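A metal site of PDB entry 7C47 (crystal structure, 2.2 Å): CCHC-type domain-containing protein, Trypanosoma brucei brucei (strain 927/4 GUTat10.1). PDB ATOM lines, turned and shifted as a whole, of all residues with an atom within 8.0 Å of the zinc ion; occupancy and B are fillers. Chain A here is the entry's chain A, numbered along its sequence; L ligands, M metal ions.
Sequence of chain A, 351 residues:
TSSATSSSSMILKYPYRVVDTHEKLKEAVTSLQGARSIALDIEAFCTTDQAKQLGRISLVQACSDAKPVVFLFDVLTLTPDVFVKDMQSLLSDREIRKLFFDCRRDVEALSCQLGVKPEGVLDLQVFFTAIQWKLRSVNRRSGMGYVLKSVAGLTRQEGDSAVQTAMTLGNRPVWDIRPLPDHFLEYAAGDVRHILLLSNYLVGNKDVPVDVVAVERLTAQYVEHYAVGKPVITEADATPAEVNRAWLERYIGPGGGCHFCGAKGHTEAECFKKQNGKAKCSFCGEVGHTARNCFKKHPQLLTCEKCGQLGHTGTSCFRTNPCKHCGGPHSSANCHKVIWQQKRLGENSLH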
ATOM      1  N   GLY A 257      18.320 -25.241  30.690  1.00  0.00           N
ATOM      2  CA  GLY A 257      16.892 -25.184  30.957  1.00  0.00           C
ATOM      3  C   GLY A 257      16.152 -24.436  29.876  1.00  0.00           C
ATOM      4  O   GLY A 257      16.745 -24.019  28.869  1.00  0.00           O
ATOM      5  N   CYS A 258      14.858 -24.241  30.097  1.00  0.00           N
ATOM      6  CA  CYS A 258      14.011 -23.618  29.092  1.00  0.00           C
ATOM      7  C   CYS A 258      14.361 -22.136  28.902  1.00  0.00           C
ATOM      8  O   CYS A 258      14.368 -21.366  29.853  1.00  0.00           O
ATOM      9  CB  CYS A 258      12.540 -23.751  29.482  1.00  0.00           C
ATOM     10  SG  CYS A 258      11.434 -23.109  28.225  1.00  0.00           S
ATOM     11  N   HIS A 259      14.647 -21.746  27.665  1.00  0.00           N
ATOM     12  CA  HIS A 259      14.950 -20.352  27.346  1.00  0.00           C
ATOM     13  C   HIS A 259      13.705 -19.463  27.389  1.00  0.00           C
ATOM     14  O   HIS A 259      13.835 -18.254  27.538  1.00  0.00           O
ATOM     15  CB  HIS A 259      15.621 -20.252  25.973  1.00  0.00           C
ATOM     16  CG  HIS A 259      16.997 -20.859  25.926  1.00  0.00           C
ATOM     17  ND1 HIS A 259      17.814 -20.773  24.824  1.00  0.00           N
ATOM     18  CD2 HIS A 259      17.701 -21.547  26.864  1.00  0.00           C
ATOM     19  CE1 HIS A 259      18.951 -21.377  25.069  1.00  0.00           C
ATOM     20  NE2 HIS A 259      18.909 -21.860  26.302  1.00  0.00           N
ATOM     21  N   PHE A 260      12.513 -20.043  27.263  1.00  0.00           N
ATOM     22  CA  PHE A 260      11.268 -19.255  27.295  1.00  0.00           C
ATOM     23  C   PHE A 260      10.813 -18.913  28.716  1.00  0.00           C
ATOM     24  O   PHE A 260      10.623 -17.737  29.033  1.00  0.00           O
ATOM     25  CB  PHE A 260      10.153 -19.977  26.537  1.00  0.00           C
ATOM     26  CG  PHE A 260       8.995 -19.074  26.222  1.00  0.00           C
ATOM     27  CD1 PHE A 260       9.076 -18.177  25.167  1.00  0.00           C
ATOM     28  CD2 PHE A 260       7.836 -19.092  27.006  1.00  0.00           C
ATOM     29  CE1 PHE A 260       8.017 -17.316  24.877  1.00  0.00           C
ATOM     30  CE2 PHE A 260       6.788 -18.236  26.726  1.00  0.00           C
ATOM     31  CZ  PHE A 260       6.869 -17.355  25.663  1.00  0.00           C
ATOM     32  N   CYS A 261      10.621 -19.932  29.556  1.00  0.00           N
ATOM     33  CA  CYS A 261      10.097 -19.756  30.926  1.00  0.00           C
ATOM     34  C   CYS A 261      11.154 -19.822  32.033  1.00  0.00           C
ATOM     35  O   CYS A 261      10.859 -19.470  33.177  1.00  0.00           O
ATOM     36  CB  CYS A 261       9.020 -20.800  31.214  1.00  0.00           C
ATOM     37  SG  CYS A 261       9.614 -22.498  31.324  1.00  0.00           S
ATOM     38  N   GLY A 262      12.362 -20.288  31.715  1.00  0.00           N
ATOM     39  CA  GLY A 262      13.465 -20.322  32.674  1.00  0.00           C
ATOM     40  C   GLY A 262      13.594 -21.591  33.511  1.00  0.00           C
ATOM     41  O   GLY A 262      14.537 -21.708  34.281  1.00  0.00           O
ATOM     42  N   ALA A 263      12.656 -22.534  33.364  1.00  0.00           N
ATOM     43  CA  ALA A 263      12.616 -23.729  34.203  1.00  0.00           C
ATOM     44  C   ALA A 263      13.536 -24.848  33.697  1.00  0.00           C
ATOM     45  O   ALA A 263      13.663 -25.061  32.479  1.00  0.00           O
ATOM     46  CB  ALA A 263      11.194 -24.252  34.315  1.00  0.00           C
ATOM     47  N   LYS A 264      14.156 -25.568  34.639  1.00  0.00           N
ATOM     48  CA  LYS A 264      14.918 -26.767  34.309  1.00  0.00           C
ATOM     49  C   LYS A 264      13.951 -27.911  33.999  1.00  0.00           C
ATOM     50  O   LYS A 264      12.808 -27.891  34.440  1.00  0.00           O
ATOM     51  CB  LYS A 264      15.832 -27.161  35.469  1.00  0.00           C
ATOM     52  CG  LYS A 264      16.888 -26.124  35.821  1.00  0.00           C
ATOM     53  CD  LYS A 264      17.650 -26.529  37.069  1.00  0.00           C
ATOM     54  CE  LYS A 264      18.421 -25.355  37.678  1.00  0.00           C
ATOM     55  NZ  LYS A 264      19.624 -24.993  36.869  1.00  0.00           N
ATOM     56  N   GLY A 265      14.411 -28.891  33.229  1.00  0.00           N
ATOM     57  CA  GLY A 265      13.638 -30.096  32.930  1.00  0.00           C
ATOM     58  C   GLY A 265      13.085 -30.199  31.518  1.00  0.00           C
ATOM     59  O   GLY A 265      12.630 -31.274  31.115  1.00  0.00           O
ATOM     60  N   HIS A 266      13.094 -29.100  30.772  1.00  0.00           N
ATOM     61  CA  HIS A 266      12.679 -29.117  29.363  1.00  0.00           C
ATOM     62  C   HIS A 266      13.278 -27.967  28.563  1.00  0.00           C
ATOM     63  O   HIS A 266      13.781 -26.994  29.133  1.00  0.00           O
ATOM     64  CB  HIS A 266      11.146 -29.088  29.250  1.00  0.00           C
ATOM     65  CG  HIS A 266      10.536 -27.813  29.740  1.00  0.00           C
ATOM     66  ND1 HIS A 266      10.318 -27.567  31.074  1.00  0.00           N
ATOM     67  CD2 HIS A 266      10.083 -26.728  29.077  1.00  0.00           C
ATOM     68  CE1 HIS A 266       9.758 -26.377  31.217  1.00  0.00           C
ATOM     69  NE2 HIS A 266       9.606 -25.852  30.020  1.00  0.00           N
ATOM     70  N   THR A 267      13.229 -28.085  27.242  1.00  0.00           N
ATOM     71  CA  THR A 267      13.710 -27.053  26.336  1.00  0.00           C
ATOM     72  C   THR A 267      12.552 -26.202  25.834  1.00  0.00           C
ATOM     73  O   THR A 267      11.382 -26.563  25.988  1.00  0.00           O
ATOM     74  CB  THR A 267      14.454 -27.648  25.125  1.00  0.00           C
ATOM     75  OG1 THR A 267      13.573 -28.533  24.410  1.00  0.00           O
ATOM     76  CG2 THR A 267      15.683 -28.403  25.578  1.00  0.00           C
ATOM     77  N   GLU A 268      12.905 -25.078  25.201  1.00  0.00           N
ATOM     78  CA  GLU A 268      11.946 -24.150  24.618  1.00  0.00           C
ATOM     79  C   GLU A 268      10.990 -24.812  23.628  1.00  0.00           C
ATOM     80  O   GLU A 268       9.802 -24.509  23.622  1.00  0.00           O
ATOM     81  CB  GLU A 268      12.692 -23.004  23.928  1.00  0.00           C
ATOM     82  CG  GLU A 268      11.820 -21.949  23.281  1.00  0.00           C
ATOM     83  CD  GLU A 268      12.603 -20.723  22.848  1.00  0.00           C
ATOM     84  OE1 GLU A 268      13.838 -20.685  23.026  1.00  0.00           O
ATOM     85  OE2 GLU A 268      11.983 -19.796  22.294  1.00  0.00           O
ATOM     86  N   ALA A 269      11.510 -25.736  22.827  1.00  0.00           N
ATOM     87  CA  ALA A 269      10.699 -26.484  21.848  1.00  0.00           C
ATOM     88  C   ALA A 269       9.614 -27.361  22.480  1.00  0.00           C
ATOM     89  O   ALA A 269       8.608 -27.649  21.839  1.00  0.00           O
ATOM     90  CB  ALA A 269      11.615 -27.326  20.967  1.00  0.00           C
ATOM     91  N   GLU A 270       9.833 -27.797  23.717  1.00  0.00           N
ATOM     92  CA  GLU A 270       8.854 -28.611  24.468  1.00  0.00           C
ATOM     93  C   GLU A 270       7.951 -27.787  25.392  1.00  0.00           C
ATOM     94  O   GLU A 270       7.052 -28.343  26.020  1.00  0.00           O
ATOM     95  CB  GLU A 270       9.604 -29.627  25.336  1.00  0.00           C
ATOM     96  CG  GLU A 270      10.612 -30.491  24.597  1.00  0.00           C
ATOM     97  CD  GLU A 270      11.497 -31.283  25.542  1.00  0.00           C
ATOM     98  OE1 GLU A 270      12.126 -30.692  26.436  1.00  0.00           O
ATOM     99  OE2 GLU A 270      11.592 -32.515  25.372  1.00  0.00           O
ATOM    100  N   CYS A 271       8.175 -26.476  25.491  1.00  0.00           N
ATOM    101  CA  CYS A 271       7.545 -25.642  26.533  1.00  0.00           C
ATOM    102  C   CYS A 271       6.050 -25.420  26.306  1.00  0.00           C
ATOM    103  O   CYS A 271       5.652 -24.859  25.279  1.00  0.00           O
ATOM    104  CB  CYS A 271       8.271 -24.298  26.624  1.00  0.00           C
ATOM    105  SG  CYS A 271       7.804 -23.278  28.027  1.00  0.00           S
ATOM    106  N   PHE A 272       5.223 -25.877  27.249  1.00  0.00           N
ATOM    107  CA  PHE A 272       3.774 -25.656  27.201  1.00  0.00           C
ATOM    108  C   PHE A 272       3.396 -24.187  27.392  1.00  0.00           C
ATOM    109  O   PHE A 272       2.457 -23.698  26.765  1.00  0.00           O
ATOM    110  CB  PHE A 272       3.023 -26.512  28.241  1.00  0.00           C
ATOM    111  CG  PHE A 272       3.161 -27.998  28.048  1.00  0.00           C
ATOM    112  CD1 PHE A 272       2.943 -28.588  26.791  1.00  0.00           C
ATOM    113  CD2 PHE A 272       3.482 -28.824  29.125  1.00  0.00           C
ATOM    114  CE1 PHE A 272       3.069 -29.966  26.624  1.00  0.00           C
ATOM    115  CE2 PHE A 272       3.598 -30.199  28.949  1.00  0.00           C
ATOM    116  CZ  PHE A 272       3.388 -30.768  27.703  1.00  0.00           C
ATOM    117  N   LYS A 273       4.121 -23.493  28.278  1.00  0.00           N
ATOM    118  CA  LYS A 273       3.885 -22.054  28.495  1.00  0.00           C
ATOM    119  C   LYS A 273       4.095 -21.221  27.234  1.00  0.00           C
ATOM    120  O   LYS A 273       3.366 -20.262  27.004  1.00  0.00           O
ATOM    121  CB  LYS A 273       4.785 -21.522  29.613  1.00  0.00           C
ATOM    122  CG  LYS A 273       4.378 -21.971  31.006  1.00  0.00           C
ATOM    123  CD  LYS A 273       5.267 -21.293  32.033  1.00  0.00           C
ATOM    124  CE  LYS A 273       4.871 -21.668  33.444  1.00  0.00           C
ATOM    125  NZ  LYS A 273       5.826 -21.070  34.407  1.00  0.00           N
ATOM    126  N   LYS A 274       5.098 -21.592  26.425  1.00  0.00           N
ATOM    127  CA  LYS A 274       5.321 -20.922  25.147  1.00  0.00           C
ATOM    128  C   LYS A 274       4.152 -21.153  24.193  1.00  0.00           C
ATOM    129  O   LYS A 274       3.629 -20.192  23.632  1.00  0.00           O
ATOM    130  CB  LYS A 274       6.619 -21.367  24.482  1.00  0.00           C
ATOM    131  CG  LYS A 274       6.982 -20.521  23.276  1.00  0.00           C
ATOM    132  CD  LYS A 274       8.232 -20.988  22.558  1.00  0.00           C
ATOM    133  CE  LYS A 274       8.523 -20.068  21.387  1.00  0.00           C
ATOM    134  NZ  LYS A 274       9.749 -20.449  20.643  1.00  0.00           N
ATOM    135  N   GLN A 275       3.743 -22.409  24.027  1.00  0.00           N
ATOM    136  CA  GLN A 275       2.670 -22.752  23.084  1.00  0.00           C
ATOM    137  C   GLN A 275       1.285 -22.244  23.530  1.00  0.00           C
ATOM    138  O   GLN A 275       0.542 -21.708  22.714  1.00  0.00           O
ATOM    139  CB  GLN A 275       2.641 -24.269  22.832  1.00  0.00           C
ATOM    140  CG  GLN A 275       1.749 -24.707  21.669  1.00  0.00           C
ATOM    141  CD  GLN A 275       2.078 -24.016  20.357  1.00  0.00           C
ATOM    142  OE1 GLN A 275       3.246 -23.751  20.043  1.00  0.00           O
ATOM    143  NE2 GLN A 275       1.041 -23.713  19.561  1.00  0.00           N
HETATM  144  O1  LIG L   1       8.870 -28.976  37.435  1.00  0.00           O
HETATM  145  P1  LIG L   1       8.025 -29.198  36.233  1.00  0.00           P
HETATM  146  O2  LIG L   1       6.613 -29.297  36.693  1.00  0.00           O
HETATM  147  O3  LIG L   1       8.609 -30.305  35.435  1.00  0.00           O
HETATM  148  O4  LIG L   1       8.187 -27.857  35.387  1.00  0.00           O
HETATM  149  C1  LIG L   1       8.187 -26.549  36.001  1.00  0.00           C
HETATM  150  C2  LIG L   1       7.347 -25.582  35.191  1.00  0.00           C
HETATM  151  O5  LIG L   1       7.570 -25.805  33.773  1.00  0.00           O
HETATM  152  C3  LIG L   1       5.837 -25.678  35.419  1.00  0.00           C
HETATM  153  O6  LIG L   1       5.263 -24.385  35.523  1.00  0.00           O
HETATM  154  C4  LIG L   1       5.342 -26.438  34.181  1.00  0.00           C
HETATM  155  O7  LIG L   1       4.019 -26.157  33.797  1.00  0.00           O
HETATM  156  C5  LIG L   1       6.331 -25.937  33.119  1.00  0.00           C
HETATM  157  N1  LIG L   1       6.505 -26.841  31.963  1.00  0.00           N
HETATM  158  C6  LIG L   1       6.217 -26.370  30.674  1.00  0.00           C
HETATM  159  N2  LIG L   1       6.385 -27.195  29.613  1.00  0.00           N
HETATM  160  C7  LIG L   1       6.826 -28.432  29.805  1.00  0.00           C
HETATM  161  C8  LIG L   1       7.126 -28.946  31.094  1.00  0.00           C
HETATM  162  C9  LIG L   1       6.953 -28.121  32.139  1.00  0.00           C
HETATM  163  O8  LIG L   1       5.820 -25.196  30.539  1.00  0.00           O
HETATM  164  N3  LIG L   1       6.977 -29.211  28.727  1.00  0.00           N
HETATM  165 ZN    ZN M   1       9.467 -23.529  29.434  1.00  0.00          ZN
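The backbone NH of Lys 273 sits at hydrogen-bond distance from an oxygen (O8) of the ligand (3.3 Å). O of Glu 270 sits at hydrogen-bond distance from N3 of the ligand, at 2.8 Å. A nitrogen (N2) of the ligand lies within hydrogen-bond range of the backbone NH (N) of Phe 272, 2.9 Å away. An oxygen (O8) of the ligand sits close to the side-chain sulfur (SG) of Cys 271, at 3.7 Å.
SG of Cys 258 lies close to N of Phe 260 (3.4 Å). The backbone NH (N) of Lys 273 sits close to the side-chain sulfur (SG) of Cys 271, at 3.7 Å. SG of Cys 261 sits close to N of Ala 263 (3.7 Å). N of Cys 258 is in hydrogen-bond range of O of Ala 263 (2.8 Å). The backbone NH (N) of Lys 274 sits close to the side-chain sulfur (SG) of Cys 271 (3.6 Å).
The nearest printed residue that does not touch the zinc ion is Phe 260 (4.6 Å).
SG of Cys 261 is bound to the zinc ion, 2.2 Å away. The zinc ion is bound by the side-chain sulfur (SG) of Cys 271. The side-chain sulfur (SG) of Cys 258 binds the zinc ion (2.3 Å). The zinc ion is bound by NE2 of His 266 (2.4 Å). The zinc ion has four donor atoms within binding distance.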
